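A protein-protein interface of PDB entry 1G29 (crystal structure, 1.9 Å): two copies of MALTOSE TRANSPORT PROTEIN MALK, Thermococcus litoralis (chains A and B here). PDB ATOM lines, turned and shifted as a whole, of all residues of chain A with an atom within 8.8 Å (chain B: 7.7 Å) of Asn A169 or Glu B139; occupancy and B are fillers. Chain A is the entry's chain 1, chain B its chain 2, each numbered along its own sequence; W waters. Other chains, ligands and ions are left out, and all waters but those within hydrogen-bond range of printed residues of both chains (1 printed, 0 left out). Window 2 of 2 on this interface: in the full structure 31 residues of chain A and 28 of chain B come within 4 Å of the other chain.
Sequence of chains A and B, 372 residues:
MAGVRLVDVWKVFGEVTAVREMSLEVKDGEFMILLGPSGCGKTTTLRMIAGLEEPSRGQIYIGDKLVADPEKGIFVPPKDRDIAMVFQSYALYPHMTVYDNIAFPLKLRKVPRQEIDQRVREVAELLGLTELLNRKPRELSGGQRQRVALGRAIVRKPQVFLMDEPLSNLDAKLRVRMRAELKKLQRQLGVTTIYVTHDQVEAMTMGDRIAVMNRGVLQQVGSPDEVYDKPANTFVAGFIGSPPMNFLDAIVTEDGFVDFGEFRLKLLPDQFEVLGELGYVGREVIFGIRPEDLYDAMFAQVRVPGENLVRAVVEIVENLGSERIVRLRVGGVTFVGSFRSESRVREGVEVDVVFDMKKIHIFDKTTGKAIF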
ATOM      1  N   GLN A  88      35.403  16.246  10.937  1.00  0.00           N
ATOM      2  CA  GLN A  88      36.336  16.243   9.790  1.00  0.00           C
ATOM      3  C   GLN A  88      36.952  14.908   9.374  1.00  0.00           C
ATOM      4  O   GLN A  88      36.417  14.193   8.530  1.00  0.00           O
ATOM      5  CB  GLN A  88      37.483  17.209  10.079  1.00  0.00           C
ATOM      6  CG  GLN A  88      37.499  18.461   9.221  1.00  0.00           C
ATOM      7  CD  GLN A  88      36.174  19.209   9.231  1.00  0.00           C
ATOM      8  OE1 GLN A  88      35.469  19.243  10.249  1.00  0.00           O
ATOM      9  NE2 GLN A  88      35.840  19.833   8.100  1.00  0.00           N
ATOM     10  N   GLN A 146      38.521   8.886   6.402  1.00  0.00           N
ATOM     11  CA  GLN A 146      37.419   9.346   7.250  1.00  0.00           C
ATOM     12  C   GLN A 146      36.634   8.135   7.789  1.00  0.00           C
ATOM     13  O   GLN A 146      36.228   8.102   8.940  1.00  0.00           O
ATOM     14  CB  GLN A 146      36.502  10.246   6.430  1.00  0.00           C
ATOM     15  CG  GLN A 146      35.737  11.279   7.253  1.00  0.00           C
ATOM     16  CD  GLN A 146      34.907  12.197   6.374  1.00  0.00           C
ATOM     17  OE1 GLN A 146      33.754  11.894   6.050  1.00  0.00           O
ATOM     18  NE2 GLN A 146      35.499  13.310   5.957  1.00  0.00           N
ATOM     19  N   ASP A 164      27.466  17.462  13.637  1.00  0.00           N
ATOM     20  CA  ASP A 164      26.854  18.737  13.280  1.00  0.00           C
ATOM     21  C   ASP A 164      26.912  18.909  11.764  1.00  0.00           C
ATOM     22  O   ASP A 164      27.914  19.364  11.208  1.00  0.00           O
ATOM     23  CB  ASP A 164      27.575  19.912  14.010  1.00  0.00           C
ATOM     24  CG  ASP A 164      26.740  21.224  13.963  1.00  0.00           C
ATOM     25  OD1 ASP A 164      25.874  21.311  13.065  1.00  0.00           O
ATOM     26  OD2 ASP A 164      26.941  22.133  14.801  1.00  0.00           O
ATOM     27  N   GLU A 165      25.829  18.491  11.116  1.00  0.00           N
ATOM     28  CA  GLU A 165      25.665  18.543   9.659  1.00  0.00           C
ATOM     29  C   GLU A 165      26.919  18.129   8.912  1.00  0.00           C
ATOM     30  O   GLU A 165      27.437  18.863   8.075  1.00  0.00           O
ATOM     31  CB  GLU A 165      25.226  19.943   9.213  1.00  0.00           C
ATOM     32  CG  GLU A 165      24.065  19.799   8.213  1.00  0.00           C
ATOM     33  CD  GLU A 165      23.562  21.088   7.649  1.00  0.00           C
ATOM     34  OE1 GLU A 165      23.007  21.932   8.394  1.00  0.00           O
ATOM     35  OE2 GLU A 165      23.738  21.255   6.422  1.00  0.00           O
ATOM     36  N   PRO A 166      27.412  16.921   9.192  1.00  0.00           N
ATOM     37  CA  PRO A 166      28.627  16.415   8.546  1.00  0.00           C
ATOM     38  C   PRO A 166      28.542  16.232   7.044  1.00  0.00           C
ATOM     39  O   PRO A 166      29.576  16.150   6.373  1.00  0.00           O
ATOM     40  CB  PRO A 166      28.880  15.089   9.276  1.00  0.00           C
ATOM     41  CG  PRO A 166      27.485  14.630   9.662  1.00  0.00           C
ATOM     42  CD  PRO A 166      26.907  15.955  10.190  1.00  0.00           C
ATOM     43  N   LEU A 167      27.328  16.174   6.516  1.00  0.00           N
ATOM     44  CA  LEU A 167      27.111  15.997   5.080  1.00  0.00           C
ATOM     45  C   LEU A 167      26.985  17.327   4.331  1.00  0.00           C
ATOM     46  O   LEU A 167      26.750  17.354   3.110  1.00  0.00           O
ATOM     47  CB  LEU A 167      25.818  15.179   4.876  1.00  0.00           C
ATOM     48  CG  LEU A 167      25.873  13.655   4.765  1.00  0.00           C
ATOM     49  CD1 LEU A 167      27.014  13.060   5.565  1.00  0.00           C
ATOM     50  CD2 LEU A 167      24.483  13.081   5.133  1.00  0.00           C
ATOM     51  N   SER A 168      27.134  18.430   5.057  1.00  0.00           N
ATOM     52  CA  SER A 168      26.986  19.764   4.486  1.00  0.00           C
ATOM     53  C   SER A 168      27.878  20.093   3.275  1.00  0.00           C
ATOM     54  O   SER A 168      27.463  20.835   2.389  1.00  0.00           O
ATOM     55  CB  SER A 168      27.227  20.796   5.569  1.00  0.00           C
ATOM     56  OG  SER A 168      28.557  20.679   6.041  1.00  0.00           O
ATOM     57  N   ASN A 169      29.082  19.533   3.256  1.00  0.00           N
ATOM     58  CA  ASN A 169      30.079  19.739   2.187  1.00  0.00           C
ATOM     59  C   ASN A 169      29.870  18.882   0.941  1.00  0.00           C
ATOM     60  O   ASN A 169      30.709  18.920   0.037  1.00  0.00           O
ATOM     61  CB  ASN A 169      31.484  19.365   2.681  1.00  0.00           C
ATOM     62  CG  ASN A 169      32.184  20.490   3.393  1.00  0.00           C
ATOM     63  OD1 ASN A 169      31.648  21.603   3.519  1.00  0.00           O
ATOM     64  ND2 ASN A 169      33.400  20.213   3.866  1.00  0.00           N
ATOM     65  N   LEU A 170      28.791  18.106   0.878  1.00  0.00           N
ATOM     66  CA  LEU A 170      28.614  17.207  -0.261  1.00  0.00           C
ATOM     67  C   LEU A 170      27.740  17.670  -1.406  1.00  0.00           C
ATOM     68  O   LEU A 170      26.790  18.416  -1.200  1.00  0.00           O
ATOM     69  CB  LEU A 170      28.071  15.884   0.244  1.00  0.00           C
ATOM     70  CG  LEU A 170      28.850  15.191   1.345  1.00  0.00           C
ATOM     71  CD1 LEU A 170      28.134  13.886   1.669  1.00  0.00           C
ATOM     72  CD2 LEU A 170      30.280  14.917   0.899  1.00  0.00           C
ATOM     73  N   ASP A 171      28.058  17.219  -2.624  1.00  0.00           N
ATOM     74  CA  ASP A 171      27.213  17.561  -3.780  1.00  0.00           C
ATOM     75  C   ASP A 171      25.855  16.888  -3.526  1.00  0.00           C
ATOM     76  O   ASP A 171      25.783  15.846  -2.884  1.00  0.00           O
ATOM     77  CB  ASP A 171      27.805  17.065  -5.125  1.00  0.00           C
ATOM     78  CG  ASP A 171      27.974  15.547  -5.196  1.00  0.00           C
ATOM     79  OD1 ASP A 171      28.966  15.047  -4.624  1.00  0.00           O
ATOM     80  OD2 ASP A 171      27.135  14.847  -5.838  1.00  0.00           O
ATOM     81  N   ALA A 172      24.796  17.487  -4.044  1.00  0.00           N
ATOM     82  CA  ALA A 172      23.449  17.001  -3.822  1.00  0.00           C
ATOM     83  C   ALA A 172      23.228  15.482  -3.929  1.00  0.00           C
ATOM     84  O   ALA A 172      22.696  14.866  -3.004  1.00  0.00           O
ATOM     85  CB  ALA A 172      22.512  17.733  -4.740  1.00  0.00           C
ATOM     86  N   LEU A 174      25.403  12.898  -3.972  1.00  0.00           N
ATOM     87  CA  LEU A 174      26.156  12.136  -3.012  1.00  0.00           C
ATOM     88  C   LEU A 174      25.519  12.304  -1.644  1.00  0.00           C
ATOM     89  O   LEU A 174      25.536  11.380  -0.851  1.00  0.00           O
ATOM     90  CB  LEU A 174      27.616  12.601  -2.955  1.00  0.00           C
ATOM     91  CG  LEU A 174      28.498  12.011  -1.866  1.00  0.00           C
ATOM     92  CD1 LEU A 174      28.585  10.501  -2.027  1.00  0.00           C
ATOM     93  CD2 LEU A 174      29.896  12.637  -1.962  1.00  0.00           C
ATOM     94  N   ARG A 175      24.972  13.484  -1.373  1.00  0.00           N
ATOM     95  CA  ARG A 175      24.349  13.731  -0.077  1.00  0.00           C
ATOM     96  C   ARG A 175      23.128  12.836   0.124  1.00  0.00           C
ATOM     97  O   ARG A 175      22.927  12.264   1.191  1.00  0.00           O
ATOM     98  CB  ARG A 175      23.948  15.196   0.034  1.00  0.00           C
ATOM     99  CG  ARG A 175      23.585  15.595   1.443  1.00  0.00           C
ATOM    100  CD  ARG A 175      23.723  17.114   1.644  1.00  0.00           C
ATOM    101  NE  ARG A 175      23.415  17.476   3.028  1.00  0.00           N
ATOM    102  CZ  ARG A 175      23.367  18.725   3.494  1.00  0.00           C
ATOM    103  NH1 ARG A 175      23.609  19.759   2.676  1.00  0.00           N
ATOM    104  NH2 ARG A 175      23.069  18.941   4.773  1.00  0.00           N
ATOM    105  N   TYR A 195      22.068  14.503  15.695  1.00  0.00           N
ATOM    106  CA  TYR A 195      22.594  15.089  14.461  1.00  0.00           C
ATOM    107  C   TYR A 195      21.906  16.430  14.250  1.00  0.00           C
ATOM    108  O   TYR A 195      20.675  16.506  14.168  1.00  0.00           O
ATOM    109  CB  TYR A 195      22.240  14.079  13.342  1.00  0.00           C
ATOM    110  CG  TYR A 195      22.669  14.365  11.915  1.00  0.00           C
ATOM    111  CD1 TYR A 195      22.114  15.423  11.180  1.00  0.00           C
ATOM    112  CD2 TYR A 195      23.630  13.557  11.290  1.00  0.00           C
ATOM    113  CE1 TYR A 195      22.503  15.668   9.872  1.00  0.00           C
ATOM    114  CE2 TYR A 195      24.031  13.786  10.005  1.00  0.00           C
ATOM    115  CZ  TYR A 195      23.472  14.856   9.291  1.00  0.00           C
ATOM    116  OH  TYR A 195      23.951  15.163   8.041  1.00  0.00           O
ATOM    117  N   HIS A 198      20.334  22.186   9.461  1.00  0.00           N
ATOM    118  CA  HIS A 198      19.423  23.312   9.207  1.00  0.00           C
ATOM    119  C   HIS A 198      18.461  22.865   8.096  1.00  0.00           C
ATOM    120  O   HIS A 198      17.526  23.558   7.794  1.00  0.00           O
ATOM    121  CB  HIS A 198      20.194  24.565   8.723  1.00  0.00           C
ATOM    122  CG  HIS A 198      20.690  24.487   7.311  1.00  0.00           C
ATOM    123  ND1 HIS A 198      21.649  23.587   6.891  1.00  0.00           N
ATOM    124  CD2 HIS A 198      20.333  25.192   6.207  1.00  0.00           C
ATOM    125  CE1 HIS A 198      21.850  23.730   5.591  1.00  0.00           C
ATOM    126  NE2 HIS A 198      21.063  24.700   5.151  1.00  0.00           N
ATOM    127  N   GLU A 202      16.507  16.948   4.954  1.00  0.00           N
ATOM    128  CA  GLU A 202      17.454  16.033   5.566  1.00  0.00           C
ATOM    129  C   GLU A 202      16.879  15.546   6.908  1.00  0.00           C
ATOM    130  O   GLU A 202      16.916  14.356   7.238  1.00  0.00           O
ATOM    131  CB  GLU A 202      18.792  16.764   5.808  1.00  0.00           C
ATOM    132  CG  GLU A 202      19.880  15.894   6.551  1.00  0.00           C
ATOM    133  CD  GLU A 202      21.255  16.455   6.270  1.00  0.00           C
ATOM    134  OE1 GLU A 202      21.660  17.442   6.908  1.00  0.00           O
ATOM    135  OE2 GLU A 202      21.903  15.950   5.361  1.00  0.00           O
ATOM    136  N   PRO B  94      29.268  25.826  12.909  1.00  0.00           N
ATOM    137  CA  PRO B  94      29.076  25.618  11.465  1.00  0.00           C
ATOM    138  C   PRO B  94      27.961  26.444  10.801  1.00  0.00           C
ATOM    139  O   PRO B  94      28.005  26.655   9.600  1.00  0.00           O
ATOM    140  CB  PRO B  94      28.807  24.092  11.339  1.00  0.00           C
ATOM    141  CG  PRO B  94      29.363  23.511  12.715  1.00  0.00           C
ATOM    142  CD  PRO B  94      28.987  24.594  13.684  1.00  0.00           C
ATOM    143  N   HIS B  95      26.974  26.902  11.566  1.00  0.00           N
ATOM    144  CA  HIS B  95      25.855  27.656  11.003  1.00  0.00           C
ATOM    145  C   HIS B  95      25.950  29.154  11.215  1.00  0.00           C
ATOM    146  O   HIS B  95      25.014  29.873  10.907  1.00  0.00           O
ATOM    147  CB  HIS B  95      24.532  27.117  11.574  1.00  0.00           C
ATOM    148  CG  HIS B  95      24.398  25.639  11.403  1.00  0.00           C
ATOM    149  ND1 HIS B  95      24.792  24.738  12.366  1.00  0.00           N
ATOM    150  CD2 HIS B  95      24.071  24.910  10.311  1.00  0.00           C
ATOM    151  CE1 HIS B  95      24.725  23.506  11.870  1.00  0.00           C
ATOM    152  NE2 HIS B  95      24.284  23.596  10.627  1.00  0.00           N
ATOM    153  N   MET B  96      27.069  29.619  11.757  1.00  0.00           N
ATOM    154  CA  MET B  96      27.276  31.073  11.935  1.00  0.00           C
ATOM    155  C   MET B  96      28.240  31.505  10.798  1.00  0.00           C
ATOM    156  O   MET B  96      29.073  30.707  10.364  1.00  0.00           O
ATOM    157  CB  MET B  96      27.943  31.358  13.304  1.00  0.00           C
ATOM    158  CG  MET B  96      27.002  31.351  14.522  1.00  0.00           C
ATOM    159  SD  MET B  96      27.828  32.127  16.017  1.00  0.00           S
ATOM    160  CE  MET B  96      29.270  32.786  15.287  1.00  0.00           C
ATOM    161  N   THR B  97      28.161  32.741  10.303  1.00  0.00           N
ATOM    162  CA  THR B  97      29.080  33.110   9.201  1.00  0.00           C
ATOM    163  C   THR B  97      30.534  33.099   9.650  1.00  0.00           C
ATOM    164  O   THR B  97      30.837  33.130  10.855  1.00  0.00           O
ATOM    165  CB  THR B  97      28.780  34.531   8.674  1.00  0.00           C
ATOM    166  OG1 THR B  97      29.008  35.455   9.744  1.00  0.00           O
ATOM    167  CG2 THR B  97      27.304  34.643   8.194  1.00  0.00           C
ATOM    168  N   VAL B  98      31.450  33.034   8.676  1.00  0.00           N
ATOM    169  CA  VAL B  98      32.873  33.047   8.984  1.00  0.00           C
ATOM    170  C   VAL B  98      33.141  34.333   9.758  1.00  0.00           C
ATOM    171  O   VAL B  98      33.875  34.360  10.771  1.00  0.00           O
ATOM    172  CB  VAL B  98      33.689  33.026   7.658  1.00  0.00           C
ATOM    173  CG1 VAL B  98      35.113  33.468   7.893  1.00  0.00           C
ATOM    174  CG2 VAL B  98      33.624  31.605   7.045  1.00  0.00           C
ATOM    175  N   LEU B 132      35.419  34.780   1.891  1.00  0.00           N
ATOM    176  CA  LEU B 132      34.582  33.799   2.595  1.00  0.00           C
ATOM    177  C   LEU B 132      33.840  34.328   3.829  1.00  0.00           C
ATOM    178  O   LEU B 132      33.095  33.580   4.490  1.00  0.00           O
ATOM    179  CB  LEU B 132      35.455  32.603   2.996  1.00  0.00           C
ATOM    180  CG  LEU B 132      36.187  31.918   1.831  1.00  0.00           C
ATOM    181  CD1 LEU B 132      37.108  30.788   2.374  1.00  0.00           C
ATOM    182  CD2 LEU B 132      35.147  31.373   0.856  1.00  0.00           C
ATOM    183  N   ASN B 134      31.137  35.979   4.411  1.00  0.00           N
ATOM    184  CA  ASN B 134      29.705  35.791   4.513  1.00  0.00           C
ATOM    185  C   ASN B 134      29.248  34.337   4.324  1.00  0.00           C
ATOM    186  O   ASN B 134      28.044  34.078   4.244  1.00  0.00           O
ATOM    187  CB  ASN B 134      28.971  36.700   3.511  1.00  0.00           C
ATOM    188  CG  ASN B 134      27.507  36.945   3.909  1.00  0.00           C
ATOM    189  OD1 ASN B 134      27.208  37.232   5.081  1.00  0.00           O
ATOM    190  ND2 ASN B 134      26.589  36.850   2.932  1.00  0.00           N
ATOM    191  N   ARG B 135      30.190  33.401   4.233  1.00  0.00           N
ATOM    192  CA  ARG B 135      29.847  31.980   4.089  1.00  0.00           C
ATOM    193  C   ARG B 135      29.807  31.372   5.508  1.00  0.00           C
ATOM    194  O   ARG B 135      30.351  31.944   6.432  1.00  0.00           O
ATOM    195  CB  ARG B 135      30.915  31.224   3.283  1.00  0.00           C
ATOM    196  CG  ARG B 135      31.194  31.782   1.875  1.00  0.00           C
ATOM    197  CD  ARG B 135      30.032  31.549   0.929  1.00  0.00           C
ATOM    198  NE  ARG B 135      28.856  32.337   1.296  1.00  0.00           N
ATOM    199  CZ  ARG B 135      27.639  32.142   0.802  1.00  0.00           C
ATOM    200  NH1 ARG B 135      27.438  31.177  -0.089  1.00  0.00           N
ATOM    201  NH2 ARG B 135      26.620  32.899   1.203  1.00  0.00           N
ATOM    202  N   LYS B 136      29.161  30.224   5.662  1.00  0.00           N
ATOM    203  CA  LYS B 136      29.105  29.550   6.961  1.00  0.00           C
ATOM    204  C   LYS B 136      30.059  28.368   6.827  1.00  0.00           C
ATOM    205  O   LYS B 136      30.155  27.740   5.763  1.00  0.00           O
ATOM    206  CB  LYS B 136      27.675  29.088   7.248  1.00  0.00           C
ATOM    207  CG  LYS B 136      26.739  30.265   7.553  1.00  0.00           C
ATOM    208  CD  LYS B 136      25.244  29.887   7.418  1.00  0.00           C
ATOM    209  CE  LYS B 136      24.346  31.124   7.596  1.00  0.00           C
ATOM    210  NZ  LYS B 136      22.894  30.794   7.429  1.00  0.00           N
ATOM    211  N   PRO B 137      30.785  28.044   7.894  1.00  0.00           N
ATOM    212  CA  PRO B 137      31.734  26.924   7.820  1.00  0.00           C
ATOM    213  C   PRO B 137      31.211  25.585   7.290  1.00  0.00           C
ATOM    214  O   PRO B 137      31.984  24.813   6.697  1.00  0.00           O
ATOM    215  CB  PRO B 137      32.263  26.826   9.250  1.00  0.00           C
ATOM    216  CG  PRO B 137      32.169  28.284   9.754  1.00  0.00           C
ATOM    217  CD  PRO B 137      30.826  28.713   9.209  1.00  0.00           C
ATOM    218  N   ARG B 138      29.910  25.321   7.469  1.00  0.00           N
ATOM    219  CA  ARG B 138      29.338  24.071   6.977  1.00  0.00           C
ATOM    220  C   ARG B 138      29.459  23.974   5.452  1.00  0.00           C
ATOM    221  O   ARG B 138      29.364  22.880   4.884  1.00  0.00           O
ATOM    222  CB  ARG B 138      27.862  23.939   7.356  1.00  0.00           C
ATOM    223  CG  ARG B 138      26.960  24.957   6.672  1.00  0.00           C
ATOM    224  CD  ARG B 138      25.503  24.871   7.110  1.00  0.00           C
ATOM    225  NE  ARG B 138      24.700  25.775   6.283  1.00  0.00           N
ATOM    226  CZ  ARG B 138      23.742  26.555   6.745  1.00  0.00           C
ATOM    227  NH1 ARG B 138      23.443  26.546   8.045  1.00  0.00           N
ATOM    228  NH2 ARG B 138      23.100  27.359   5.899  1.00  0.00           N
ATOM    229  N   GLU B 139      29.653  25.108   4.797  1.00  0.00           N
ATOM    230  CA  GLU B 139      29.764  25.119   3.336  1.00  0.00           C
ATOM    231  C   GLU B 139      31.220  25.087   2.854  1.00  0.00           C
ATOM    232  O   GLU B 139      31.468  24.905   1.652  1.00  0.00           O
ATOM    233  CB  GLU B 139      29.130  26.395   2.757  1.00  0.00           C
ATOM    234  CG  GLU B 139      27.656  26.641   3.013  1.00  0.00           C
ATOM    235  CD  GLU B 139      27.246  28.043   2.555  1.00  0.00           C
ATOM    236  OE1 GLU B 139      27.802  29.033   3.093  1.00  0.00           O
ATOM    237  OE2 GLU B 139      26.376  28.162   1.653  1.00  0.00           O
ATOM    238  N   LEU B 140      32.178  25.268   3.763  1.00  0.00           N
ATOM    239  CA  LEU B 140      33.580  25.325   3.348  1.00  0.00           C
ATOM    240  C   LEU B 140      34.353  24.002   3.325  1.00  0.00           C
ATOM    241  O   LEU B 140      33.932  23.003   3.908  1.00  0.00           O
ATOM    242  CB  LEU B 140      34.328  26.333   4.229  1.00  0.00           C
ATOM    243  CG  LEU B 140      33.611  27.690   4.349  1.00  0.00           C
ATOM    244  CD1 LEU B 140      34.408  28.668   5.192  1.00  0.00           C
ATOM    245  CD2 LEU B 140      33.376  28.249   2.961  1.00  0.00           C
ATOM    246  N   SER B 141      35.508  24.031   2.665  1.00  0.00           N
ATOM    247  CA  SER B 141      36.380  22.866   2.584  1.00  0.00           C
ATOM    248  C   SER B 141      37.073  22.731   3.922  1.00  0.00           C
ATOM    249  O   SER B 141      37.104  23.678   4.728  1.00  0.00           O
ATOM    250  CB  SER B 141      37.450  23.079   1.503  1.00  0.00           C
ATOM    251  OG  SER B 141      38.415  24.037   1.950  1.00  0.00           O
ATOM    252  N   GLY B 142      37.659  21.561   4.157  1.00  0.00           N
ATOM    253  CA  GLY B 142      38.369  21.333   5.406  1.00  0.00           C
ATOM    254  C   GLY B 142      39.496  22.337   5.645  1.00  0.00           C
ATOM    255  O   GLY B 142      39.649  22.845   6.759  1.00  0.00           O
ATOM    256  N   GLY B 143      40.273  22.625   4.600  1.00  0.00           N
ATOM    257  CA  GLY B 143      41.389  23.566   4.723  1.00  0.00           C
ATOM    258  C   GLY B 143      40.907  24.967   5.054  1.00  0.00           C
ATOM    259  O   GLY B 143      41.535  25.686   5.850  1.00  0.00           O
ATOM    260  N   GLN B 144      39.814  25.375   4.411  1.00  0.00           N
ATOM    261  CA  GLN B 144      39.241  26.688   4.667  1.00  0.00           C
ATOM    262  C   GLN B 144      38.750  26.768   6.128  1.00  0.00           C
ATOM    263  O   GLN B 144      38.931  27.784   6.810  1.00  0.00           O
ATOM    264  CB  GLN B 144      38.098  26.937   3.686  1.00  0.00           C
ATOM    265  CG  GLN B 144      38.632  27.094   2.254  1.00  0.00           C
ATOM    266  CD  GLN B 144      37.563  27.366   1.220  1.00  0.00           C
ATOM    267  OE1 GLN B 144      37.818  28.040   0.207  1.00  0.00           O
ATOM    268  NE2 GLN B 144      36.369  26.821   1.441  1.00  0.00           N
ATOM    269  N   ARG B 145      38.114  25.700   6.607  1.00  0.00           N
ATOM    270  CA  ARG B 145      37.656  25.688   7.999  1.00  0.00           C
ATOM    271  C   ARG B 145      38.831  25.801   8.977  1.00  0.00           C
ATOM    272  O   ARG B 145      38.744  26.510   9.988  1.00  0.00           O
ATOM    273  CB  ARG B 145      36.880  24.408   8.329  1.00  0.00           C
ATOM    274  CG  ARG B 145      35.454  24.371   7.782  1.00  0.00           C
ATOM    275  CD  ARG B 145      34.621  23.228   8.386  1.00  0.00           C
ATOM    276  NE  ARG B 145      33.839  22.585   7.342  1.00  0.00           N
ATOM    277  CZ  ARG B 145      32.679  21.948   7.513  1.00  0.00           C
ATOM    278  NH1 ARG B 145      32.118  21.850   8.721  1.00  0.00           N
ATOM    279  NH2 ARG B 145      32.073  21.411   6.454  1.00  0.00           N
HETATM  280  O   HOH W   1      28.954  21.046   9.030  1.00  0.00           O
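A ring nitrogen (NE2) of His A198 lies within hydrogen-bond range of the guanidinium group of Arg B138, 3.4 Å away.
The side-chain amide oxygen (OD1) of Asn A169 sits close to the backbone carbonyl oxygen (O) of Leu B140, at 2.7 Å.
NE2 of Gln A88 lies close to NE of Arg B145 (3.5 Å).
OD1 of Asn A169 sits close to O of Arg B138, at 3.0 Å.
The side-chain carboxylate (OE1) of Glu A165 is in hydrogen-bond range of a ring nitrogen (NE2) of His B95.
The side-chain amide oxygen (OD1) of Asn A169 lies within hydrogen-bond range of the guanidinium group (NH2) of Arg B145, at 3.0 Å.
The side-chain hydroxyl (OG) of Ser A168 is in hydrogen-bond range of the backbone carbonyl oxygen (O) of Arg B138 (2.6 Å).
The backbone carbonyl oxygen (O) of Gln A88 sits at hydrogen-bond distance from the side-chain amide nitrogen (NE2) of Gln A146, at 2.9 Å.
O of Pro B137 sits at hydrogen-bond distance from NE of Arg B145 (3.0 Å).
The guanidinium group of Arg B135 lies within salt-bridge range of the side-chain carboxylate of Glu B139 (3.6 Å).
The backbone carbonyl oxygen (O) of Arg B138 is in hydrogen-bond range of the guanidinium group (NH2) of Arg B145.
The backbone carbonyl oxygen (O) of Glu A165 sits at hydrogen-bond distance from the side-chain hydroxyl (OG) of Ser A168, 2.9 Å away.
NE of Arg B145 is in hydrogen-bond range of O of Leu B140 (3.5 Å).
Of chain B, only Arg B138, Glu B139, Leu B140 and Arg B145 come within 4 Å of Asn A169.
Of the printed residues of chain A, Glu B139 touches Asn A169.
Ser A168 touches just these residues of chain B: Arg B138 (2.6 Å) and Arg B145 (3.6 Å).
Of the printed residues of chain B, His A198 touches Arg B138.
Of the printed residues of chain A, Arg B138 touches Ser A168, Asn A169 and His A198.
Printed residues of chain A within 4 Å of Arg B145: Gln A88, Ser A168 and Asn A169.
Printed residues of chain B within 4 Å of Glu A165: His B95.
Printed residues of chain A within 4 Å of His B95: Asp A164 and Glu A165.
The nearest residue of chain A that does not touch Glu B139 is Ser A168 (4.7 Å).
No position is printed for both chains.
Of the 12 pairs that touch across the chains among the printed residues, none has its exchanged pair printed and touching as well.
Water W1 lies within hydrogen-bond range of the backbone carbonyl oxygen of Glu A165, the backbone carbonyl oxygen of Asp A164, the side-chain hydroxyl of Ser A168 and the guanidinium group of Arg B145.
Of the 16 printed residues of chain A, 6 touch a printed residue of chain B.
Hydrophobic or aromatic side chains of chain A that line the printed part of chain B: His A198.
Of the 18 printed residues of chain B, 7 touch a printed residue of chain A.
Printed residues of chain B that touch a printed residue of chain A: Pro B94, His B95, Arg B138, Glu B139, Leu B140, Gly B142 and Arg B145.
Among the printed residues, 12 pairs touch across the chains.
Among the printed residues, no Asp or Glu carboxylate lies within 4 Å of a Lys or Arg side-chain nitrogen of the other chain.
CA of Gly B142 touches NE2 of Gln A88, at 3.99 Å.
CD of Pro B94 touches OD2 of Asp A164, at 3.4 Å.
Asp A164 touches His B95.
OG of Ser A168 touches NH2 of Arg B145, at 3.6 Å.
OD1 of Asn A169 touches C of Glu B139, 3.6 Å away.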
